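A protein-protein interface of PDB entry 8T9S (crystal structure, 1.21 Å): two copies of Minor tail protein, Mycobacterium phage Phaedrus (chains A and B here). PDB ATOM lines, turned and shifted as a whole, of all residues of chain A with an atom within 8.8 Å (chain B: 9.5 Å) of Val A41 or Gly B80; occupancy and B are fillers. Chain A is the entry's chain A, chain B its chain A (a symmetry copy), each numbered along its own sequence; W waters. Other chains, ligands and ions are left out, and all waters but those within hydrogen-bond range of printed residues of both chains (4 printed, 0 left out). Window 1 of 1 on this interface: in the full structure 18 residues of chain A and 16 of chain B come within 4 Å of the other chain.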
ATOM      1  N   GLY A  38      32.576  14.804   0.456  1.00  0.00           N
ATOM      2  CA  GLY A  38      31.971  13.720  -0.286  1.00  0.00           C
ATOM      3  C   GLY A  38      30.693  13.221   0.345  1.00  0.00           C
ATOM      4  O   GLY A  38      30.430  13.435   1.532  1.00  0.00           O
ATOM      5  N   ILE A  39      29.913  12.523  -0.468  1.00  0.00           N
ATOM      6  CA  ILE A  39      28.740  11.806  -0.012  1.00  0.00           C
ATOM      7  C   ILE A  39      28.749  10.435  -0.669  1.00  0.00           C
ATOM      8  O   ILE A  39      28.981  10.319  -1.875  1.00  0.00           O
ATOM      9  CB  ILE A  39      27.441  12.548  -0.367  1.00  0.00           C
ATOM     10  CG1 ILE A  39      27.490  13.950   0.221  1.00  0.00           C
ATOM     11  CG2 ILE A  39      26.231  11.767   0.140  1.00  0.00           C
ATOM     12  CD1 ILE A  39      26.299  14.839  -0.219  1.00  0.00           C
ATOM     13  N   ASP A  40      28.461   9.400   0.122  1.00  0.00           N
ATOM     14  CA  ASP A  40      28.348   8.032  -0.353  1.00  0.00           C
ATOM     15  C   ASP A  40      27.014   7.497   0.131  1.00  0.00           C
ATOM     16  O   ASP A  40      26.658   7.664   1.300  1.00  0.00           O
ATOM     17  CB  ASP A  40      29.510   7.192   0.145  1.00  0.00           C
ATOM     18  CG  ASP A  40      30.845   7.663  -0.464  1.00  0.00           C
ATOM     19  OD1 ASP A  40      31.124   7.344  -1.658  1.00  0.00           O
ATOM     20  OD2 ASP A  40      31.610   8.413   0.220  1.00  0.00           O
ATOM     21  N   VAL A  41      26.271   6.879  -0.784  1.00  0.00           N
ATOM     22  CA  VAL A  41      24.991   6.243  -0.483  1.00  0.00           C
ATOM     23  C   VAL A  41      25.044   4.807  -0.979  1.00  0.00           C
ATOM     24  O   VAL A  41      25.413   4.545  -2.131  1.00  0.00           O
ATOM     25  CB  VAL A  41      23.809   6.996  -1.126  1.00  0.00           C
ATOM     26  CG1 VAL A  41      22.521   6.345  -0.742  1.00  0.00           C
ATOM     27  CG2 VAL A  41      23.817   8.435  -0.698  1.00  0.00           C
ATOM     28  N   THR A  42      24.686   3.875  -0.117  1.00  0.00           N
ATOM     29  CA  THR A  42      24.546   2.483  -0.542  1.00  0.00           C
ATOM     30  C   THR A  42      23.127   2.008  -0.302  1.00  0.00           C
ATOM     31  O   THR A  42      22.525   2.285   0.759  1.00  0.00           O
ATOM     32  CB  THR A  42      25.545   1.551   0.168  1.00  0.00           C
ATOM     33  OG1 THR A  42      25.290   1.561   1.569  1.00  0.00           O
ATOM     34  CG2 THR A  42      26.980   1.997  -0.058  1.00  0.00           C
ATOM     35  N   TRP A  43      22.594   1.306  -1.303  1.00  0.00           N
ATOM     36  CA  TRP A  43      21.351   0.550  -1.180  1.00  0.00           C
ATOM     37  C   TRP A  43      21.710  -0.925  -1.228  1.00  0.00           C
ATOM     38  O   TRP A  43      22.247  -1.398  -2.240  1.00  0.00           O
ATOM     39  CB  TRP A  43      20.369   0.868  -2.316  1.00  0.00           C
ATOM     40  CG  TRP A  43      19.168  -0.026  -2.316  1.00  0.00           C
ATOM     41  CD1 TRP A  43      18.894  -1.049  -3.197  1.00  0.00           C
ATOM     42  CD2 TRP A  43      18.076  -0.014  -1.362  1.00  0.00           C
ATOM     43  NE1 TRP A  43      17.698  -1.654  -2.848  1.00  0.00           N
ATOM     44  CE2 TRP A  43      17.186  -1.035  -1.730  1.00  0.00           C
ATOM     45  CE3 TRP A  43      17.774   0.765  -0.239  1.00  0.00           C
ATOM     46  CZ2 TRP A  43      16.035  -1.286  -1.016  1.00  0.00           C
ATOM     47  CZ3 TRP A  43      16.635   0.513   0.436  1.00  0.00           C
ATOM     48  CH2 TRP A  43      15.782  -0.510   0.056  1.00  0.00           C
ATOM     49  N   SER A  44      21.413  -1.640  -0.149  1.00  0.00           N
ATOM     50  CA  SER A  44      21.600  -3.078  -0.089  1.00  0.00           C
ATOM     51  C   SER A  44      20.236  -3.725  -0.255  1.00  0.00           C
ATOM     52  O   SER A  44      19.349  -3.527   0.599  1.00  0.00           O
ATOM     53  CB  SER A  44      22.152  -3.511   1.267  1.00  0.00           C
ATOM     54  OG  SER A  44      23.429  -2.958   1.447  1.00  0.00           O
ATOM     55  N   GLU A  45      20.082  -4.506  -1.330  1.00  0.00           N
ATOM     56  CA  GLU A  45      18.850  -5.239  -1.583  1.00  0.00           C
ATOM     57  C   GLU A  45      18.608  -6.243  -0.471  1.00  0.00           C
ATOM     58  O   GLU A  45      19.537  -6.764   0.147  1.00  0.00           O
ATOM     59  CB  GLU A  45      18.959  -6.042  -2.891  1.00  0.00           C
ATOM     60  CG  GLU A  45      19.245  -5.210  -4.106  1.00  0.00           C
ATOM     61  CD  GLU A  45      19.683  -6.088  -5.276  1.00  0.00           C
ATOM     62  OE1 GLU A  45      19.387  -7.310  -5.248  1.00  0.00           O
ATOM     63  OE2 GLU A  45      20.345  -5.560  -6.212  1.00  0.00           O
ATOM     64  N   GLU A  62      18.936  -2.243   3.328  1.00  0.00           N
ATOM     65  CA  GLU A  62      19.533  -1.158   4.079  1.00  0.00           C
ATOM     66  C   GLU A  62      19.797   0.012   3.148  1.00  0.00           C
ATOM     67  O   GLU A  62      20.235  -0.171   2.010  1.00  0.00           O
ATOM     68  CB  GLU A  62      20.864  -1.582   4.716  1.00  0.00           C
ATOM     69  CG  GLU A  62      20.742  -2.734   5.724  1.00  0.00           C
ATOM     70  CD  GLU A  62      22.073  -3.034   6.458  1.00  0.00           C
ATOM     71  OE1 GLU A  62      23.162  -2.630   5.960  1.00  0.00           O
ATOM     72  OE2 GLU A  62      22.032  -3.676   7.538  1.00  0.00           O
ATOM     73  N   LEU A  63      19.547   1.226   3.643  1.00  0.00           N
ATOM     74  CA  LEU A  63      19.867   2.469   2.939  1.00  0.00           C
ATOM     75  C   LEU A  63      20.747   3.289   3.877  1.00  0.00           C
ATOM     76  O   LEU A  63      20.334   3.613   4.994  1.00  0.00           O
ATOM     77  CB  LEU A  63      18.579   3.210   2.589  1.00  0.00           C
ATOM     78  CG  LEU A  63      18.724   4.541   1.854  1.00  0.00           C
ATOM     79  CD1 LEU A  63      19.474   4.358   0.550  1.00  0.00           C
ATOM     80  CD2 LEU A  63      17.343   5.154   1.603  1.00  0.00           C
ATOM     81  N   THR A  64      21.949   3.616   3.433  1.00  0.00           N
ATOM     82  CA  THR A  64      22.925   4.283   4.271  1.00  0.00           C
ATOM     83  C   THR A  64      23.530   5.457   3.537  1.00  0.00           C
ATOM     84  O   THR A  64      23.952   5.318   2.386  1.00  0.00           O
ATOM     85  CB  THR A  64      24.014   3.270   4.643  1.00  0.00           C
ATOM     86  OG1 THR A  64      23.383   2.120   5.252  1.00  0.00           O
ATOM     87  CG2 THR A  64      25.051   3.890   5.613  1.00  0.00           C
ATOM     88  N   VAL A  65      23.564   6.611   4.197  1.00  0.00           N
ATOM     89  CA  VAL A  65      24.123   7.836   3.648  1.00  0.00           C
ATOM     90  C   VAL A  65      25.288   8.247   4.532  1.00  0.00           C
ATOM     91  O   VAL A  65      25.097   8.508   5.723  1.00  0.00           O
ATOM     92  CB  VAL A  65      23.081   8.960   3.599  1.00  0.00           C
ATOM     93  CG1 VAL A  65      23.734  10.275   3.101  1.00  0.00           C
ATOM     94  CG2 VAL A  65      21.913   8.562   2.726  1.00  0.00           C
ATOM     95  N   THR A  66      26.484   8.302   3.959  1.00  0.00           N
ATOM     96  CA  THR A  66      27.696   8.673   4.687  1.00  0.00           C
ATOM     97  C   THR A  66      28.276   9.958   4.117  1.00  0.00           C
ATOM     98  O   THR A  66      28.562  10.031   2.920  1.00  0.00           O
ATOM     99  CB  THR A  66      28.729   7.540   4.591  1.00  0.00           C
ATOM    100  OG1 THR A  66      28.159   6.327   5.104  1.00  0.00           O
ATOM    101  CG2 THR A  66      29.977   7.876   5.398  1.00  0.00           C
ATOM    102  N   VAL A  67      28.458  10.964   4.982  1.00  0.00           N
ATOM    103  CA  VAL A  67      29.073  12.243   4.623  1.00  0.00           C
ATOM    104  C   VAL A  67      30.528  12.232   5.076  1.00  0.00           C
ATOM    105  O   VAL A  67      30.817  11.929   6.236  1.00  0.00           O
ATOM    106  CB  VAL A  67      28.305  13.427   5.254  1.00  0.00           C
ATOM    107  CG1 VAL A  67      28.923  14.760   4.837  1.00  0.00           C
ATOM    108  CG2 VAL A  67      26.840  13.384   4.890  1.00  0.00           C
ATOM    109  N   HIS A  76      27.224   9.519   9.509  1.00  0.00           N
ATOM    110  CA  HIS A  76      26.005   9.086   8.835  1.00  0.00           C
ATOM    111  C   HIS A  76      24.945  10.198   8.884  1.00  0.00           C
ATOM    112  O   HIS A  76      24.758  10.869   9.918  1.00  0.00           O
ATOM    113  CB  HIS A  76      25.442   7.822   9.497  1.00  0.00           C
ATOM    114  CG  HIS A  76      26.284   6.590   9.302  1.00  0.00           C
ATOM    115  ND1 HIS A  76      26.723   6.157   8.061  1.00  0.00           N
ATOM    116  CD2 HIS A  76      26.746   5.672  10.194  1.00  0.00           C
ATOM    117  CE1 HIS A  76      27.438   5.046   8.205  1.00  0.00           C
ATOM    118  NE2 HIS A  76      27.462   4.727   9.485  1.00  0.00           N
ATOM    119  N   ALA A  77      24.257  10.402   7.761  1.00  0.00           N
ATOM    120  CA  ALA A  77      23.079  11.252   7.701  1.00  0.00           C
ATOM    121  C   ALA A  77      21.826  10.383   7.650  1.00  0.00           C
ATOM    122  O   ALA A  77      21.844   9.235   7.188  1.00  0.00           O
ATOM    123  CB  ALA A  77      23.075  12.158   6.454  1.00  0.00           C
ATOM    124  N   PRO A  79      18.667   9.013   6.036  1.00  0.00           N
ATOM    125  CA  PRO A  79      18.217   8.968   4.640  1.00  0.00           C
ATOM    126  C   PRO A  79      16.898   9.652   4.419  1.00  0.00           C
ATOM    127  O   PRO A  79      16.663  10.207   3.346  1.00  0.00           O
ATOM    128  CB  PRO A  79      18.115   7.458   4.343  1.00  0.00           C
ATOM    129  CG  PRO A  79      19.037   6.791   5.340  1.00  0.00           C
ATOM    130  CD  PRO A  79      18.935   7.651   6.580  1.00  0.00           C
ATOM    131  N   CYS A  82      17.463  13.338   4.114  1.00  0.00           N
ATOM    132  CA  CYS A  82      18.073  13.649   2.827  1.00  0.00           C
ATOM    133  C   CYS A  82      17.015  13.699   1.741  1.00  0.00           C
ATOM    134  O   CYS A  82      16.977  14.644   0.946  1.00  0.00           O
ATOM    135  CB  CYS A  82      19.116  12.583   2.493  1.00  0.00           C
ATOM    136  SG  CYS A  82      20.607  12.664   3.540  1.00  0.00           S
ATOM    137  N   ILE A  83      16.159  12.670   1.672  1.00  0.00           N
ATOM    138  CA  ILE A  83      15.158  12.622   0.620  1.00  0.00           C
ATOM    139  C   ILE A  83      14.142  13.726   0.827  1.00  0.00           C
ATOM    140  O   ILE A  83      13.678  14.367  -0.136  1.00  0.00           O
ATOM    141  CB  ILE A  83      14.518  11.228   0.575  1.00  0.00           C
ATOM    142  CG1 ILE A  83      15.576  10.203   0.145  1.00  0.00           C
ATOM    143  CG2 ILE A  83      13.335  11.208  -0.402  1.00  0.00           C
ATOM    144  CD1 ILE A  83      15.120   8.778   0.297  1.00  0.00           C
ATOM    145  N   LEU A  86      15.683  16.998  -0.513  1.00  0.00           N
ATOM    146  CA  LEU A  86      15.660  17.013  -1.979  1.00  0.00           C
ATOM    147  C   LEU A  86      14.269  17.376  -2.503  1.00  0.00           C
ATOM    148  O   LEU A  86      14.131  18.191  -3.430  1.00  0.00           O
ATOM    149  CB  LEU A  86      16.097  15.651  -2.525  1.00  0.00           C
ATOM    150  CG  LEU A  86      17.552  15.295  -2.347  1.00  0.00           C
ATOM    151  CD1 LEU A  86      17.776  13.845  -2.778  1.00  0.00           C
ATOM    152  CD2 LEU A  86      18.433  16.261  -3.135  1.00  0.00           C
ATOM    153  N   PHE B   6      24.773  15.305 -14.941  1.00  0.00           N
ATOM    154  CA  PHE B   6      23.996  14.192 -14.406  1.00  0.00           C
ATOM    155  C   PHE B   6      23.683  13.193 -15.503  1.00  0.00           C
ATOM    156  O   PHE B   6      23.813  11.974 -15.315  1.00  0.00           O
ATOM    157  CB  PHE B   6      22.714  14.689 -13.709  1.00  0.00           C
ATOM    158  CG  PHE B   6      22.132  13.674 -12.762  1.00  0.00           C
ATOM    159  CD1 PHE B   6      21.353  12.645 -13.236  1.00  0.00           C
ATOM    160  CD2 PHE B   6      22.393  13.733 -11.388  1.00  0.00           C
ATOM    161  CE1 PHE B   6      20.849  11.680 -12.366  1.00  0.00           C
ATOM    162  CE2 PHE B   6      21.903  12.788 -10.514  1.00  0.00           C
ATOM    163  CZ  PHE B   6      21.140  11.750 -10.999  1.00  0.00           C
ATOM    164  N   HIS B  13      27.105   5.288 -15.920  1.00  0.00           N
ATOM    165  CA  HIS B  13      26.729   4.283 -14.922  1.00  0.00           C
ATOM    166  C   HIS B  13      26.056   3.064 -15.558  1.00  0.00           C
ATOM    167  O   HIS B  13      26.396   1.915 -15.231  1.00  0.00           O
ATOM    168  CB  HIS B  13      25.817   4.924 -13.872  1.00  0.00           C
ATOM    169  CG  HIS B  13      25.284   3.957 -12.858  1.00  0.00           C
ATOM    170  ND1 HIS B  13      26.081   3.381 -11.896  1.00  0.00           N
ATOM    171  CD2 HIS B  13      24.028   3.491 -12.627  1.00  0.00           C
ATOM    172  CE1 HIS B  13      25.350   2.594 -11.120  1.00  0.00           C
ATOM    173  NE2 HIS B  13      24.097   2.648 -11.539  1.00  0.00           N
ATOM    174  N   ARG B  17      26.478  -1.615 -16.935  1.00  0.00           N
ATOM    175  CA  ARG B  17      25.514  -2.581 -16.422  1.00  0.00           C
ATOM    176  C   ARG B  17      24.727  -3.274 -17.524  1.00  0.00           C
ATOM    177  O   ARG B  17      23.778  -4.021 -17.233  1.00  0.00           O
ATOM    178  CB  ARG B  17      24.572  -1.865 -15.449  1.00  0.00           C
ATOM    179  CG  ARG B  17      25.310  -1.148 -14.350  1.00  0.00           C
ATOM    180  CD  ARG B  17      24.394  -0.242 -13.553  1.00  0.00           C
ATOM    181  NE  ARG B  17      23.419  -0.983 -12.767  1.00  0.00           N
ATOM    182  CZ  ARG B  17      23.665  -1.498 -11.579  1.00  0.00           C
ATOM    183  NH1 ARG B  17      24.874  -1.435 -11.035  1.00  0.00           N
ATOM    184  NH2 ARG B  17      22.674  -2.090 -10.921  1.00  0.00           N
ATOM    185  N   LEU B  63      13.533  -1.485  -3.838  1.00  0.00           N
ATOM    186  CA  LEU B  63      13.680  -0.208  -4.538  1.00  0.00           C
ATOM    187  C   LEU B  63      14.381  -0.511  -5.858  1.00  0.00           C
ATOM    188  O   LEU B  63      15.493  -1.045  -5.865  1.00  0.00           O
ATOM    189  CB  LEU B  63      14.493   0.760  -3.682  1.00  0.00           C
ATOM    190  CG  LEU B  63      14.753   2.148  -4.263  1.00  0.00           C
ATOM    191  CD1 LEU B  63      13.449   2.854  -4.577  1.00  0.00           C
ATOM    192  CD2 LEU B  63      15.595   2.975  -3.288  1.00  0.00           C
ATOM    193  N   THR B  64      13.737  -0.179  -6.965  1.00  0.00           N
ATOM    194  CA  THR B  64      14.236  -0.526  -8.280  1.00  0.00           C
ATOM    195  C   THR B  64      14.190   0.679  -9.192  1.00  0.00           C
ATOM    196  O   THR B  64      13.164   1.358  -9.270  1.00  0.00           O
ATOM    197  CB  THR B  64      13.365  -1.654  -8.846  1.00  0.00           C
ATOM    198  OG1 THR B  64      13.356  -2.746  -7.897  1.00  0.00           O
ATOM    199  CG2 THR B  64      13.893  -2.139 -10.218  1.00  0.00           C
ATOM    200  N   VAL B  65      15.302   0.946  -9.871  1.00  0.00           N
ATOM    201  CA  VAL B  65      15.428   2.056 -10.802  1.00  0.00           C
ATOM    202  C   VAL B  65      15.716   1.474 -12.176  1.00  0.00           C
ATOM    203  O   VAL B  65      16.736   0.805 -12.361  1.00  0.00           O
ATOM    204  CB  VAL B  65      16.555   3.012 -10.391  1.00  0.00           C
ATOM    205  CG1 VAL B  65      16.726   4.127 -11.455  1.00  0.00           C
ATOM    206  CG2 VAL B  65      16.284   3.594  -9.023  1.00  0.00           C
ATOM    207  N   ALA B  77      19.592   0.700 -12.885  1.00  0.00           N
ATOM    208  CA  ALA B  77      20.610   1.508 -12.230  1.00  0.00           C
ATOM    209  C   ALA B  77      20.627   1.193 -10.738  1.00  0.00           C
ATOM    210  O   ALA B  77      19.624   0.775 -10.145  1.00  0.00           O
ATOM    211  CB  ALA B  77      20.348   3.019 -12.390  1.00  0.00           C
ATOM    212  N   ASP B  78      21.756   1.447 -10.126  1.00  0.00           N
ATOM    213  CA  ASP B  78      21.870   1.220  -8.686  1.00  0.00           C
ATOM    214  C   ASP B  78      21.165   2.343  -7.920  1.00  0.00           C
ATOM    215  O   ASP B  78      21.482   3.526  -8.133  1.00  0.00           O
ATOM    216  CB  ASP B  78      23.325   1.146  -8.293  1.00  0.00           C
ATOM    217  CG  ASP B  78      23.505   0.765  -6.878  1.00  0.00           C
ATOM    218  OD1 ASP B  78      23.327   1.589  -6.010  1.00  0.00           O
ATOM    219  OD2 ASP B  78      23.792  -0.405  -6.628  1.00  0.00           O
ATOM    220  N   PRO B  79      20.202   2.027  -7.052  1.00  0.00           N
ATOM    221  CA  PRO B  79      19.474   3.101  -6.365  1.00  0.00           C
ATOM    222  C   PRO B  79      20.350   3.942  -5.482  1.00  0.00           C
ATOM    223  O   PRO B  79      20.097   5.134  -5.316  1.00  0.00           O
ATOM    224  CB  PRO B  79      18.415   2.344  -5.537  1.00  0.00           C
ATOM    225  CG  PRO B  79      18.236   1.014  -6.236  1.00  0.00           C
ATOM    226  CD  PRO B  79      19.609   0.687  -6.778  1.00  0.00           C
ATOM    227  N   GLY B  80      21.377   3.337  -4.901  1.00  0.00           N
ATOM    228  CA  GLY B  80      22.294   4.099  -4.067  1.00  0.00           C
ATOM    229  C   GLY B  80      23.092   5.116  -4.855  1.00  0.00           C
ATOM    230  O   GLY B  80      23.234   6.274  -4.429  1.00  0.00           O
ATOM    231  N   TRP B  81      23.622   4.699  -6.017  1.00  0.00           N
ATOM    232  CA  TRP B  81      24.307   5.629  -6.905  1.00  0.00           C
ATOM    233  C   TRP B  81      23.378   6.793  -7.278  1.00  0.00           C
ATOM    234  O   TRP B  81      23.783   7.966  -7.301  1.00  0.00           O
ATOM    235  CB  TRP B  81      24.765   4.860  -8.147  1.00  0.00           C
ATOM    236  CG  TRP B  81      25.525   5.678  -9.116  1.00  0.00           C
ATOM    237  CD1 TRP B  81      26.878   5.741  -9.254  1.00  0.00           C
ATOM    238  CD2 TRP B  81      24.983   6.562 -10.104  1.00  0.00           C
ATOM    239  NE1 TRP B  81      27.216   6.618 -10.260  1.00  0.00           N
ATOM    240  CE2 TRP B  81      26.073   7.144 -10.787  1.00  0.00           C
ATOM    241  CE3 TRP B  81      23.672   6.919 -10.482  1.00  0.00           C
ATOM    242  CZ2 TRP B  81      25.900   8.059 -11.799  1.00  0.00           C
ATOM    243  CZ3 TRP B  81      23.506   7.839 -11.491  1.00  0.00           C
ATOM    244  CH2 TRP B  81      24.601   8.402 -12.132  1.00  0.00           C
ATOM    245  N   CYS B  82      22.121   6.487  -7.575  1.00  0.00           N
ATOM    246  CA  CYS B  82      21.191   7.530  -7.992  1.00  0.00           C
ATOM    247  C   CYS B  82      21.002   8.544  -6.880  1.00  0.00           C
ATOM    248  O   CYS B  82      21.074   9.754  -7.116  1.00  0.00           O
ATOM    249  CB  CYS B  82      19.850   6.893  -8.354  1.00  0.00           C
ATOM    250  SG  CYS B  82      19.894   5.918  -9.896  1.00  0.00           S
ATOM    251  N   ILE B  83      20.728   8.068  -5.657  1.00  0.00           N
ATOM    252  CA  ILE B  83      20.476   8.982  -4.557  1.00  0.00           C
ATOM    253  C   ILE B  83      21.744   9.732  -4.211  1.00  0.00           C
ATOM    254  O   ILE B  83      21.720  10.941  -3.907  1.00  0.00           O
ATOM    255  CB  ILE B  83      19.897   8.211  -3.363  1.00  0.00           C
ATOM    256  CG1 ILE B  83      18.512   7.670  -3.738  1.00  0.00           C
ATOM    257  CG2 ILE B  83      19.795   9.121  -2.132  1.00  0.00           C
ATOM    258  CD1 ILE B  83      17.959   6.701  -2.728  1.00  0.00           C
ATOM    259  N   GLU B  84      22.879   9.041  -4.273  1.00  0.00           N
ATOM    260  CA  GLU B  84      24.134   9.710  -3.976  1.00  0.00           C
ATOM    261  C   GLU B  84      24.344  10.886  -4.898  1.00  0.00           C
ATOM    262  O   GLU B  84      24.770  11.964  -4.461  1.00  0.00           O
ATOM    263  CB  GLU B  84      25.293   8.743  -4.127  1.00  0.00           C
ATOM    264  CG  GLU B  84      26.642   9.416  -3.930  1.00  0.00           C
ATOM    265  CD  GLU B  84      27.801   8.429  -4.004  1.00  0.00           C
ATOM    266  OE1 GLU B  84      27.648   7.248  -3.512  1.00  0.00           O
ATOM    267  OE2 GLU B  84      28.867   8.844  -4.558  1.00  0.00           O
ATOM    268  N   ASN B  85      24.110  10.686  -6.189  1.00  0.00           N
ATOM    269  CA  ASN B  85      24.401  11.752  -7.136  1.00  0.00           C
ATOM    270  C   ASN B  85      23.392  12.874  -7.124  1.00  0.00           C
ATOM    271  O   ASN B  85      23.762  14.012  -7.406  1.00  0.00           O
ATOM    272  CB  ASN B  85      24.666  11.154  -8.486  1.00  0.00           C
ATOM    273  CG  ASN B  85      26.054  10.538  -8.540  1.00  0.00           C
ATOM    274  OD1 ASN B  85      27.056  11.268  -8.572  1.00  0.00           O
ATOM    275  ND2 ASN B  85      26.124   9.208  -8.447  1.00  0.00           N
ATOM    276  N   LEU B  86      22.143  12.596  -6.763  1.00  0.00           N
ATOM    277  CA  LEU B  86      21.209  13.685  -6.462  1.00  0.00           C
ATOM    278  C   LEU B  86      21.728  14.551  -5.312  1.00  0.00           C
ATOM    279  O   LEU B  86      21.681  15.790  -5.376  1.00  0.00           O
ATOM    280  CB  LEU B  86      19.830  13.116  -6.122  1.00  0.00           C
ATOM    281  CG  LEU B  86      19.060  12.498  -7.263  1.00  0.00           C
ATOM    282  CD1 LEU B  86      17.801  11.823  -6.720  1.00  0.00           C
ATOM    283  CD2 LEU B  86      18.727  13.557  -8.309  1.00  0.00           C
ATOM    284  N   LEU B  87      22.193  13.907  -4.229  1.00  0.00           N
ATOM    285  CA  LEU B  87      22.702  14.646  -3.076  1.00  0.00           C
ATOM    286  C   LEU B  87      23.978  15.385  -3.417  1.00  0.00           C
ATOM    287  O   LEU B  87      24.169  16.533  -2.987  1.00  0.00           O
ATOM    288  CB  LEU B  87      22.942  13.689  -1.899  1.00  0.00           C
ATOM    289  CG  LEU B  87      21.668  13.116  -1.283  1.00  0.00           C
ATOM    290  CD1 LEU B  87      22.037  12.010  -0.312  1.00  0.00           C
ATOM    291  CD2 LEU B  87      20.847  14.192  -0.581  1.00  0.00           C
ATOM    292  N   ARG B  88      24.870  14.764  -4.179  1.00  0.00           N
ATOM    293  CA  ARG B  88      26.087  15.464  -4.575  1.00  0.00           C
ATOM    294  C   ARG B  88      25.763  16.757  -5.332  1.00  0.00           C
ATOM    295  O   ARG B  88      26.297  17.831  -5.018  1.00  0.00           O
ATOM    296  CB  ARG B  88      26.950  14.531  -5.419  1.00  0.00           C
ATOM    297  CG  ARG B  88      27.687  13.477  -4.592  1.00  0.00           C
ATOM    298  CD  ARG B  88      28.492  12.520  -5.445  1.00  0.00           C
ATOM    299  NE  ARG B  88      29.430  11.787  -4.588  1.00  0.00           N
ATOM    300  CZ  ARG B  88      30.626  12.257  -4.206  1.00  0.00           C
ATOM    301  NH1 ARG B  88      31.104  13.420  -4.660  1.00  0.00           N
ATOM    302  NH2 ARG B  88      31.355  11.557  -3.341  1.00  0.00           N
HETATM  303  O   HOH W   1      15.687  -3.602  -3.742  1.00  0.00           O
HETATM  304  O   HOH W   2      24.340   0.979  -3.544  1.00  0.00           O
HETATM  305  O   HOH W   3      22.154  -1.818  -4.772  1.00  0.00           O
HETATM  306  O   HOH W   4      27.158   4.585  -4.774  1.00  0.00           O
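The guanidinium group (NH2) of Arg B88 is in hydrogen-bond range of the backbone carbonyl oxygen (O) of Ile A39, 3.1 Å away. The side-chain carboxylate (OE2) of Glu B84 lies close to the backbone carbonyl oxygen (O) of Ile A39 (3.1 Å). N of Val A41 lies within hydrogen-bond range of OE1 of Glu B84 (3.1 Å).
Arg B88 touches Gly A38 (NH2 to CA, 3.8 Å). Ile A39 touches Leu B87 (CD1 to O, 3.9 Å). OE1 of Glu B84 touches CA of Asp A40, at 3.3 Å. Val A41 touches Gly B80. Trp A43 touches Leu B63. Pro B79 touches Trp A43 (CG to CD1, 3.7 Å). CB of Trp A43 touches N of Gly B80 (3.7 Å). CD2 of Leu B87 touches CB of Cys A82, 3.9 Å away. CD2 of Leu A86 touches O of Leu B86, 3.97 Å away. CD1 of Leu A86 touches CD2 of Leu B87, 3.8 Å away.
Of the printed residues of chain B, Val A41 touches Gly B80 (3.4 Å) and Glu B84 (3.1 Å). No residue of chain B comes within 4 Å of Thr A42. Pro B79 touches just one residue of chain A: Trp A43 (3.7 Å). Of the printed residues of chain B, Ile A39 touches Glu B84 (3.1 Å), Leu B87 (3.9 Å) and Arg B88 (3.1 Å). Of the printed residues of chain B, Gly A38 touches Arg B88 (3.8 Å). Ser A44 touches none of the printed residues of chain B. The nearest printed residue of chain B that does not touch Val A41 is Leu B87 (4.01 Å). The nearest residue of chain A that does not touch Gly B80 is Thr A42 (4.4 Å). The nearest printed residue of chain B that does not touch Cys A82 is Ile B83 (5.8 Å).
Of the 20 printed residues of chain A, 7 touch a printed residue of chain B. Along chain A the printed residues that touch a printed residue of chain B span positions 38 to 86. Of the 18 printed residues of chain B, 7 touch a printed residue of chain A. Printed residues of chain B that touch a printed residue of chain A: Leu B63, Pro B79, Gly B80, Glu B84, Leu B86, Leu B87 and Arg B88. Hydrophobic or aromatic side chains of chain B that line the printed part of chain A: Leu B63, Pro B79, Leu B86 and Leu B87. Among the printed residues, no Asp or Glu carboxylate lies within 4 Å of a Lys or Arg side-chain nitrogen of the other chain.
Leu A86 touches its own counterpart, Leu B86. Of the 13 pairs that touch across the chains among the printed residues, 1 has its exchanged pair printed and touching as well.
OD1 of Asp B78 sits at hydrogen-bond distance from N of Gly B80 (2.8 Å). The side-chain carboxylate (OE2) of Glu B84 lies within salt-bridge range of the guanidinium group (NE) of Arg B88 (3.0 Å). O of Asp A40 lies within hydrogen-bond range of N of Thr A66 (2.7 Å).
Water W3 lies within hydrogen-bond range of the backbone carbonyl oxygen of Trp A43 (2.6 Å) and the side-chain carboxylate of Asp B78 (2.9 Å). Water W2 bridges the side-chain carboxylate (OD1) of Asp B78 (2.7 Å) and the backbone NH (N) of Trp A43 (2.9 Å). Water W1 lies within hydrogen-bond range of NE1 of Trp A43 and N of Leu B63. Water W4 lies within hydrogen-bond range of OE1 of Glu B84 and O of Val A41.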
